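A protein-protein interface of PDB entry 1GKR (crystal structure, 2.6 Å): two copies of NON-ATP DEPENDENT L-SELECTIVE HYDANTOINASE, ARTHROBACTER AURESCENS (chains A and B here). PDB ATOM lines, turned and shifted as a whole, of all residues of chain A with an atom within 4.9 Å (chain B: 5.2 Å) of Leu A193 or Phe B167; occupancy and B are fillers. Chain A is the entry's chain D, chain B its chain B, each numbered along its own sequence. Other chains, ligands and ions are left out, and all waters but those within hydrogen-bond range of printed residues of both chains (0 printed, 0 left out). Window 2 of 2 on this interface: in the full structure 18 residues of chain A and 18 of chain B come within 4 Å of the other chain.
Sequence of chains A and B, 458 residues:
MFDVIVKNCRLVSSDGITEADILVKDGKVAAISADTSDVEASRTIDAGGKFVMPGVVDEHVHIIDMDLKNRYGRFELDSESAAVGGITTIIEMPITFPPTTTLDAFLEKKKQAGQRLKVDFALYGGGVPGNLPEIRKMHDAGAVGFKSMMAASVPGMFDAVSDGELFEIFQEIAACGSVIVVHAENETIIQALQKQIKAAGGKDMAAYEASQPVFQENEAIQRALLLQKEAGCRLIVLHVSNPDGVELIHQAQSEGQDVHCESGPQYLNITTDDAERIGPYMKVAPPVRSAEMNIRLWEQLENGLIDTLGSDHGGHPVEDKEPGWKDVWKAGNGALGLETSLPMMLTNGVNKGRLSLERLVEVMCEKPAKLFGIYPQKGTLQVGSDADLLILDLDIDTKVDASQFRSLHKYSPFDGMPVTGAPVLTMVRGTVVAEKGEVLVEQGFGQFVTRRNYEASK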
ATOM      1  N   ILE A 189      18.962  -1.331 -17.332  1.00  0.00           N
ATOM      2  CA  ILE A 189      19.545  -2.329 -18.223  1.00  0.00           C
ATOM      3  C   ILE A 189      19.555  -3.666 -17.511  1.00  0.00           C
ATOM      4  O   ILE A 189      19.297  -4.704 -18.118  1.00  0.00           O
ATOM      5  CB  ILE A 189      20.976  -1.940 -18.629  1.00  0.00           C
ATOM      6  CG1 ILE A 189      20.910  -0.809 -19.661  1.00  0.00           C
ATOM      7  CG2 ILE A 189      21.730  -3.156 -19.176  1.00  0.00           C
ATOM      8  CD1 ILE A 189      22.232  -0.138 -19.918  1.00  0.00           C
ATOM      9  N   ILE A 190      19.838  -3.642 -16.216  1.00  0.00           N
ATOM     10  CA  ILE A 190      19.844  -4.868 -15.446  1.00  0.00           C
ATOM     11  C   ILE A 190      18.461  -5.501 -15.528  1.00  0.00           C
ATOM     12  O   ILE A 190      18.343  -6.705 -15.744  1.00  0.00           O
ATOM     13  CB  ILE A 190      20.216  -4.609 -13.991  1.00  0.00           C
ATOM     14  CG1 ILE A 190      21.682  -4.200 -13.920  1.00  0.00           C
ATOM     15  CG2 ILE A 190      19.998  -5.857 -13.166  1.00  0.00           C
ATOM     16  CD1 ILE A 190      22.166  -3.877 -12.532  1.00  0.00           C
ATOM     17  N   GLN A 191      17.413  -4.698 -15.376  1.00  0.00           N
ATOM     18  CA  GLN A 191      16.060  -5.233 -15.460  1.00  0.00           C
ATOM     19  C   GLN A 191      15.809  -5.880 -16.814  1.00  0.00           C
ATOM     20  O   GLN A 191      15.297  -7.000 -16.884  1.00  0.00           O
ATOM     21  CB  GLN A 191      15.029  -4.135 -15.261  1.00  0.00           C
ATOM     22  CG  GLN A 191      14.968  -3.580 -13.866  1.00  0.00           C
ATOM     23  CD  GLN A 191      13.961  -2.450 -13.754  1.00  0.00           C
ATOM     24  OE1 GLN A 191      13.930  -1.734 -12.752  1.00  0.00           O
ATOM     25  NE2 GLN A 191      13.129  -2.282 -14.787  1.00  0.00           N
ATOM     26  N   ALA A 192      16.163  -5.177 -17.887  1.00  0.00           N
ATOM     27  CA  ALA A 192      15.958  -5.707 -19.229  1.00  0.00           C
ATOM     28  C   ALA A 192      16.703  -7.019 -19.413  1.00  0.00           C
ATOM     29  O   ALA A 192      16.138  -8.000 -19.901  1.00  0.00           O
ATOM     30  CB  ALA A 192      16.408  -4.703 -20.276  1.00  0.00           C
ATOM     31  N   LEU A 193      17.970  -7.042 -19.029  1.00  0.00           N
ATOM     32  CA  LEU A 193      18.744  -8.259 -19.164  1.00  0.00           C
ATOM     33  C   LEU A 193      18.176  -9.396 -18.299  1.00  0.00           C
ATOM     34  O   LEU A 193      18.179 -10.552 -18.716  1.00  0.00           O
ATOM     35  CB  LEU A 193      20.200  -7.988 -18.804  1.00  0.00           C
ATOM     36  CG  LEU A 193      20.901  -7.069 -19.793  1.00  0.00           C
ATOM     37  CD1 LEU A 193      22.285  -6.761 -19.287  1.00  0.00           C
ATOM     38  CD2 LEU A 193      20.956  -7.733 -21.156  1.00  0.00           C
ATOM     39  N   GLN A 194      17.688  -9.076 -17.104  1.00  0.00           N
ATOM     40  CA  GLN A 194      17.123 -10.111 -16.242  1.00  0.00           C
ATOM     41  C   GLN A 194      15.989 -10.823 -16.946  1.00  0.00           C
ATOM     42  O   GLN A 194      15.904 -12.051 -16.915  1.00  0.00           O
ATOM     43  CB  GLN A 194      16.582  -9.513 -14.955  1.00  0.00           C
ATOM     44  CG  GLN A 194      17.551  -9.526 -13.811  1.00  0.00           C
ATOM     45  CD  GLN A 194      17.018  -8.776 -12.614  1.00  0.00           C
ATOM     46  OE1 GLN A 194      17.666  -8.716 -11.579  1.00  0.00           O
ATOM     47  NE2 GLN A 194      15.830  -8.194 -12.755  1.00  0.00           N
ATOM     48  N   LYS A 195      15.111 -10.040 -17.569  1.00  0.00           N
ATOM     49  CA  LYS A 195      13.977 -10.602 -18.281  1.00  0.00           C
ATOM     50  C   LYS A 195      14.444 -11.476 -19.421  1.00  0.00           C
ATOM     51  O   LYS A 195      13.979 -12.599 -19.554  1.00  0.00           O
ATOM     52  CB  LYS A 195      13.050  -9.501 -18.800  1.00  0.00           C
ATOM     53  CG  LYS A 195      12.365  -8.740 -17.679  1.00  0.00           C
ATOM     54  CD  LYS A 195      11.149  -7.936 -18.146  1.00  0.00           C
ATOM     55  CE  LYS A 195      10.421  -7.292 -16.940  1.00  0.00           C
ATOM     56  NZ  LYS A 195       9.100  -6.649 -17.263  1.00  0.00           N
ATOM     57  N   GLN A 196      15.372 -10.987 -20.233  1.00  0.00           N
ATOM     58  CA  GLN A 196      15.848 -11.791 -21.349  1.00  0.00           C
ATOM     59  C   GLN A 196      16.437 -13.102 -20.831  1.00  0.00           C
ATOM     60  O   GLN A 196      16.065 -14.177 -21.297  1.00  0.00           O
ATOM     61  CB  GLN A 196      16.916 -11.049 -22.161  1.00  0.00           C
ATOM     62  CG  GLN A 196      16.542  -9.636 -22.597  1.00  0.00           C
ATOM     63  CD  GLN A 196      17.449  -9.098 -23.707  1.00  0.00           C
ATOM     64  OE1 GLN A 196      18.631  -9.453 -23.795  1.00  0.00           O
ATOM     65  NE2 GLN A 196      16.895  -8.226 -24.551  1.00  0.00           N
ATOM     66  N   ILE A 197      17.344 -13.005 -19.861  1.00  0.00           N
ATOM     67  CA  ILE A 197      18.001 -14.180 -19.290  1.00  0.00           C
ATOM     68  C   ILE A 197      17.055 -15.147 -18.586  1.00  0.00           C
ATOM     69  O   ILE A 197      17.187 -16.362 -18.743  1.00  0.00           O
ATOM     70  CB  ILE A 197      19.141 -13.758 -18.334  1.00  0.00           C
ATOM     71  CG1 ILE A 197      20.321 -13.242 -19.159  1.00  0.00           C
ATOM     72  CG2 ILE A 197      19.590 -14.927 -17.481  1.00  0.00           C
ATOM     73  CD1 ILE A 197      21.418 -12.611 -18.347  1.00  0.00           C
ATOM     74  N   LYS A 198      16.111 -14.625 -17.810  1.00  0.00           N
ATOM     75  CA  LYS A 198      15.159 -15.495 -17.133  1.00  0.00           C
ATOM     76  C   LYS A 198      14.329 -16.227 -18.180  1.00  0.00           C
ATOM     77  O   LYS A 198      14.107 -17.432 -18.079  1.00  0.00           O
ATOM     78  CB  LYS A 198      14.246 -14.695 -16.195  1.00  0.00           C
ATOM     79  CG  LYS A 198      14.701 -14.738 -14.742  1.00  0.00           C
ATOM     80  CD  LYS A 198      13.789 -13.951 -13.822  1.00  0.00           C
ATOM     81  CE  LYS A 198      14.511 -12.760 -13.215  1.00  0.00           C
ATOM     82  NZ  LYS A 198      13.616 -11.937 -12.342  1.00  0.00           N
ATOM     83  N   ALA A 210      25.749 -12.544 -15.852  1.00  0.00           N
ATOM     84  CA  ALA A 210      25.411 -12.031 -17.173  1.00  0.00           C
ATOM     85  C   ALA A 210      24.304 -10.999 -17.152  1.00  0.00           C
ATOM     86  O   ALA A 210      24.224 -10.178 -18.061  1.00  0.00           O
ATOM     87  CB  ALA A 210      25.026 -13.161 -18.087  1.00  0.00           C
ATOM     88  N   SER A 211      23.452 -11.040 -16.129  1.00  0.00           N
ATOM     89  CA  SER A 211      22.343 -10.089 -16.036  1.00  0.00           C
ATOM     90  C   SER A 211      22.809  -8.700 -15.581  1.00  0.00           C
ATOM     91  O   SER A 211      22.080  -7.715 -15.715  1.00  0.00           O
ATOM     92  CB  SER A 211      21.243 -10.625 -15.100  1.00  0.00           C
ATOM     93  OG  SER A 211      21.657 -10.661 -13.748  1.00  0.00           O
ATOM     94  N   PRO A 213      26.225  -7.402 -16.421  1.00  0.00           N
ATOM     95  CA  PRO A 213      27.538  -7.401 -17.081  1.00  0.00           C
ATOM     96  C   PRO A 213      28.404  -6.184 -16.807  1.00  0.00           C
ATOM     97  O   PRO A 213      27.919  -5.174 -16.296  1.00  0.00           O
ATOM     98  CB  PRO A 213      27.182  -7.548 -18.563  1.00  0.00           C
ATOM     99  CG  PRO A 213      25.866  -6.878 -18.656  1.00  0.00           C
ATOM    100  CD  PRO A 213      25.145  -7.367 -17.424  1.00  0.00           C
ATOM    101  N   PHE A 215      29.746  -4.108 -18.947  1.00  0.00           N
ATOM    102  CA  PHE A 215      29.443  -2.948 -19.767  1.00  0.00           C
ATOM    103  C   PHE A 215      28.436  -2.017 -19.106  1.00  0.00           C
ATOM    104  O   PHE A 215      28.522  -0.798 -19.272  1.00  0.00           O
ATOM    105  CB  PHE A 215      29.017  -3.376 -21.176  1.00  0.00           C
ATOM    106  CG  PHE A 215      27.545  -3.527 -21.362  1.00  0.00           C
ATOM    107  CD1 PHE A 215      26.731  -2.406 -21.513  1.00  0.00           C
ATOM    108  CD2 PHE A 215      26.970  -4.788 -21.433  1.00  0.00           C
ATOM    109  CE1 PHE A 215      25.363  -2.536 -21.735  1.00  0.00           C
ATOM    110  CE2 PHE A 215      25.596  -4.938 -21.653  1.00  0.00           C
ATOM    111  CZ  PHE A 215      24.791  -3.811 -21.805  1.00  0.00           C
ATOM    112  N   SER B 162      13.762   4.308 -21.438  1.00  0.00           N
ATOM    113  CA  SER B 162      14.789   4.265 -20.409  1.00  0.00           C
ATOM    114  C   SER B 162      15.989   3.561 -21.032  1.00  0.00           C
ATOM    115  O   SER B 162      15.895   3.043 -22.147  1.00  0.00           O
ATOM    116  CB  SER B 162      14.307   3.477 -19.202  1.00  0.00           C
ATOM    117  OG  SER B 162      13.972   2.154 -19.568  1.00  0.00           O
ATOM    118  N   ASP B 163      17.115   3.524 -20.330  1.00  0.00           N
ATOM    119  CA  ASP B 163      18.290   2.866 -20.894  1.00  0.00           C
ATOM    120  C   ASP B 163      18.013   1.401 -21.238  1.00  0.00           C
ATOM    121  O   ASP B 163      18.474   0.905 -22.256  1.00  0.00           O
ATOM    122  CB  ASP B 163      19.488   3.001 -19.947  1.00  0.00           C
ATOM    123  CG  ASP B 163      19.841   4.458 -19.668  1.00  0.00           C
ATOM    124  OD1 ASP B 163      19.580   5.296 -20.544  1.00  0.00           O
ATOM    125  OD2 ASP B 163      20.382   4.780 -18.588  1.00  0.00           O
ATOM    126  N   GLY B 164      17.229   0.719 -20.415  1.00  0.00           N
ATOM    127  CA  GLY B 164      16.911  -0.676 -20.672  1.00  0.00           C
ATOM    128  C   GLY B 164      16.060  -0.825 -21.918  1.00  0.00           C
ATOM    129  O   GLY B 164      16.314  -1.686 -22.767  1.00  0.00           O
ATOM    130  N   GLU B 165      15.046   0.019 -22.051  1.00  0.00           N
ATOM    131  CA  GLU B 165      14.181  -0.057 -23.223  1.00  0.00           C
ATOM    132  C   GLU B 165      14.992   0.313 -24.457  1.00  0.00           C
ATOM    133  O   GLU B 165      14.885  -0.330 -25.505  1.00  0.00           O
ATOM    134  CB  GLU B 165      12.987   0.887 -23.058  1.00  0.00           C
ATOM    135  CG  GLU B 165      12.396   0.834 -21.669  1.00  0.00           C
ATOM    136  CD  GLU B 165      11.082   1.553 -21.558  1.00  0.00           C
ATOM    137  OE1 GLU B 165      10.062   0.962 -21.962  1.00  0.00           O
ATOM    138  OE2 GLU B 165      11.070   2.705 -21.074  1.00  0.00           O
ATOM    139  N   LEU B 166      15.808   1.357 -24.322  1.00  0.00           N
ATOM    140  CA  LEU B 166      16.658   1.802 -25.414  1.00  0.00           C
ATOM    141  C   LEU B 166      17.610   0.672 -25.809  1.00  0.00           C
ATOM    142  O   LEU B 166      17.844   0.426 -26.992  1.00  0.00           O
ATOM    143  CB  LEU B 166      17.466   3.031 -24.998  1.00  0.00           C
ATOM    144  CG  LEU B 166      18.377   3.617 -26.087  1.00  0.00           C
ATOM    145  CD1 LEU B 166      17.555   4.000 -27.315  1.00  0.00           C
ATOM    146  CD2 LEU B 166      19.096   4.820 -25.542  1.00  0.00           C
ATOM    147  N   PHE B 167      18.156  -0.023 -24.817  1.00  0.00           N
ATOM    148  CA  PHE B 167      19.062  -1.126 -25.098  1.00  0.00           C
ATOM    149  C   PHE B 167      18.366  -2.258 -25.844  1.00  0.00           C
ATOM    150  O   PHE B 167      18.937  -2.840 -26.769  1.00  0.00           O
ATOM    151  CB  PHE B 167      19.661  -1.673 -23.812  1.00  0.00           C
ATOM    152  CG  PHE B 167      20.646  -2.771 -24.041  1.00  0.00           C
ATOM    153  CD1 PHE B 167      21.862  -2.508 -24.666  1.00  0.00           C
ATOM    154  CD2 PHE B 167      20.350  -4.074 -23.672  1.00  0.00           C
ATOM    155  CE1 PHE B 167      22.772  -3.528 -24.921  1.00  0.00           C
ATOM    156  CE2 PHE B 167      21.249  -5.103 -23.920  1.00  0.00           C
ATOM    157  CZ  PHE B 167      22.465  -4.829 -24.548  1.00  0.00           C
ATOM    158  N   GLU B 168      17.136  -2.575 -25.447  1.00  0.00           N
ATOM    159  CA  GLU B 168      16.401  -3.652 -26.115  1.00  0.00           C
ATOM    160  C   GLU B 168      16.090  -3.264 -27.554  1.00  0.00           C
ATOM    161  O   GLU B 168      16.087  -4.107 -28.454  1.00  0.00           O
ATOM    162  CB  GLU B 168      15.103  -3.971 -25.374  1.00  0.00           C
ATOM    163  CG  GLU B 168      15.331  -4.522 -23.985  1.00  0.00           C
ATOM    164  CD  GLU B 168      14.060  -5.043 -23.347  1.00  0.00           C
ATOM    165  OE1 GLU B 168      13.040  -4.305 -23.333  1.00  0.00           O
ATOM    166  OE2 GLU B 168      14.098  -6.195 -22.850  1.00  0.00           O
ATOM    167  N   ILE B 169      15.828  -1.975 -27.765  1.00  0.00           N
ATOM    168  CA  ILE B 169      15.531  -1.480 -29.097  1.00  0.00           C
ATOM    169  C   ILE B 169      16.785  -1.611 -29.948  1.00  0.00           C
ATOM    170  O   ILE B 169      16.706  -2.031 -31.095  1.00  0.00           O
ATOM    171  CB  ILE B 169      15.067  -0.020 -29.043  1.00  0.00           C
ATOM    172  CG1 ILE B 169      13.717   0.046 -28.335  1.00  0.00           C
ATOM    173  CG2 ILE B 169      14.990   0.573 -30.451  1.00  0.00           C
ATOM    174  CD1 ILE B 169      13.171   1.461 -28.166  1.00  0.00           C
ATOM    175  N   PHE B 170      17.942  -1.269 -29.377  1.00  0.00           N
ATOM    176  CA  PHE B 170      19.211  -1.371 -30.095  1.00  0.00           C
ATOM    177  C   PHE B 170      19.424  -2.806 -30.554  1.00  0.00           C
ATOM    178  O   PHE B 170      19.831  -3.045 -31.697  1.00  0.00           O
ATOM    179  CB  PHE B 170      20.375  -0.961 -29.203  1.00  0.00           C
ATOM    180  CG  PHE B 170      20.639   0.527 -29.168  1.00  0.00           C
ATOM    181  CD1 PHE B 170      19.698   1.436 -29.636  1.00  0.00           C
ATOM    182  CD2 PHE B 170      21.820   1.013 -28.624  1.00  0.00           C
ATOM    183  CE1 PHE B 170      19.935   2.810 -29.556  1.00  0.00           C
ATOM    184  CE2 PHE B 170      22.062   2.378 -28.544  1.00  0.00           C
ATOM    185  CZ  PHE B 170      21.115   3.278 -29.011  1.00  0.00           C
ATOM    186  N   GLN B 171      19.148  -3.768 -29.678  1.00  0.00           N
ATOM    187  CA  GLN B 171      19.312  -5.164 -30.063  1.00  0.00           C
ATOM    188  C   GLN B 171      18.367  -5.549 -31.187  1.00  0.00           C
ATOM    189  O   GLN B 171      18.785  -6.225 -32.125  1.00  0.00           O
ATOM    190  CB  GLN B 171      19.089  -6.084 -28.881  1.00  0.00           C
ATOM    191  CG  GLN B 171      20.052  -5.850 -27.758  1.00  0.00           C
ATOM    192  CD  GLN B 171      19.800  -6.776 -26.595  1.00  0.00           C
ATOM    193  OE1 GLN B 171      18.655  -6.952 -26.152  1.00  0.00           O
ATOM    194  NE2 GLN B 171      20.868  -7.373 -26.082  1.00  0.00           N
ATOM    195  N   LEU B 227      26.066   2.120 -25.223  1.00  0.00           N
ATOM    196  CA  LEU B 227      25.084   1.074 -25.461  1.00  0.00           C
ATOM    197  C   LEU B 227      25.173   0.534 -26.876  1.00  0.00           C
ATOM    198  O   LEU B 227      24.935  -0.647 -27.088  1.00  0.00           O
ATOM    199  CB  LEU B 227      23.656   1.574 -25.202  1.00  0.00           C
ATOM    200  CG  LEU B 227      23.373   2.208 -23.835  1.00  0.00           C
ATOM    201  CD1 LEU B 227      21.881   2.237 -23.595  1.00  0.00           C
ATOM    202  CD2 LEU B 227      24.034   1.413 -22.755  1.00  0.00           C
ATOM    203  N   GLU B 230      27.861  -1.971 -27.330  1.00  0.00           N
ATOM    204  CA  GLU B 230      27.483  -3.311 -26.900  1.00  0.00           C
ATOM    205  C   GLU B 230      26.461  -3.991 -27.817  1.00  0.00           C
ATOM    206  O   GLU B 230      26.484  -5.198 -27.974  1.00  0.00           O
ATOM    207  CB  GLU B 230      26.908  -3.231 -25.495  1.00  0.00           C
ATOM    208  CG  GLU B 230      26.799  -4.542 -24.784  1.00  0.00           C
ATOM    209  CD  GLU B 230      28.155  -5.084 -24.373  1.00  0.00           C
ATOM    210  OE1 GLU B 230      29.137  -4.285 -24.337  1.00  0.00           O
ATOM    211  OE2 GLU B 230      28.225  -6.305 -24.078  1.00  0.00           O
ATOM    212  N   ALA B 231      25.562  -3.221 -28.418  1.00  0.00           N
ATOM    213  CA  ALA B 231      24.538  -3.785 -29.292  1.00  0.00           C
ATOM    214  C   ALA B 231      24.962  -3.988 -30.745  1.00  0.00           C
ATOM    215  O   ALA B 231      24.493  -4.916 -31.393  1.00  0.00           O
ATOM    216  CB  ALA B 231      23.293  -2.907 -29.250  1.00  0.00           C
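Ile A189 touches Asp B163 (CG1 to O, 3.95 Å).
Gly B164 touches Ile A189.
Ile A189 touches Leu B227.
Gly B164 touches Ala A192 (O to CB, 3.9 Å).
Ala A192 touches Glu B168.
Phe B167 touches Leu A193.
Gln A196 touches Glu B168 (NE2 to OE2, 3.9 Å).
CZ of Phe A215 touches CE1 of Phe B167, at 3.7 Å.
Phe A215 touches Glu B230 (CD2 to CD, 3.2 Å).
The side-chain amide nitrogen (NE2) of Gln A196 sits at hydrogen-bond distance from the side-chain amide oxygen (OE1) of Gln B171 (2.7 Å).
Of the printed residues of chain B, Ile A189 touches Asp B163, Gly B164 and Leu B227.
Of the printed residues of chain B, Ala A192 touches Gly B164 and Glu B168.
Leu A193 touches just one residue of chain B: Phe B167 (3.8 Å).
Printed residues of chain B within 4 Å of Gln A196: Glu B168 (3.9 Å) and Gln B171 (2.7 Å).
Phe B167 touches just these residues of chain A: Leu A193 and Phe A215.
Phe B170 touches none of the printed residues of chain A.
Of the printed residues of chain A, Leu B227 touches Ile A189.
Printed residues of chain A within 4 Å of Glu B230: Phe A215 (3.2 Å).
The nearest residue of chain B that does not touch Leu A193 is Gln B171 (4.9 Å).
The nearest printed residue of chain A that does not touch Asp B163 is Ala A192 (6.3 Å).
No position is printed for both chains.
Hydrophobic or aromatic side chains of chain A that line the printed part of chain B: Ile A189, Ala A192, Leu A193 and Phe A215.
Hydrophobic or aromatic side chains of chain B that line the printed part of chain A: Phe B167 and Leu B227.
Among the printed residues, no Asp or Glu carboxylate lies within 4 Å of a Lys or Arg side-chain nitrogen of the other chain.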
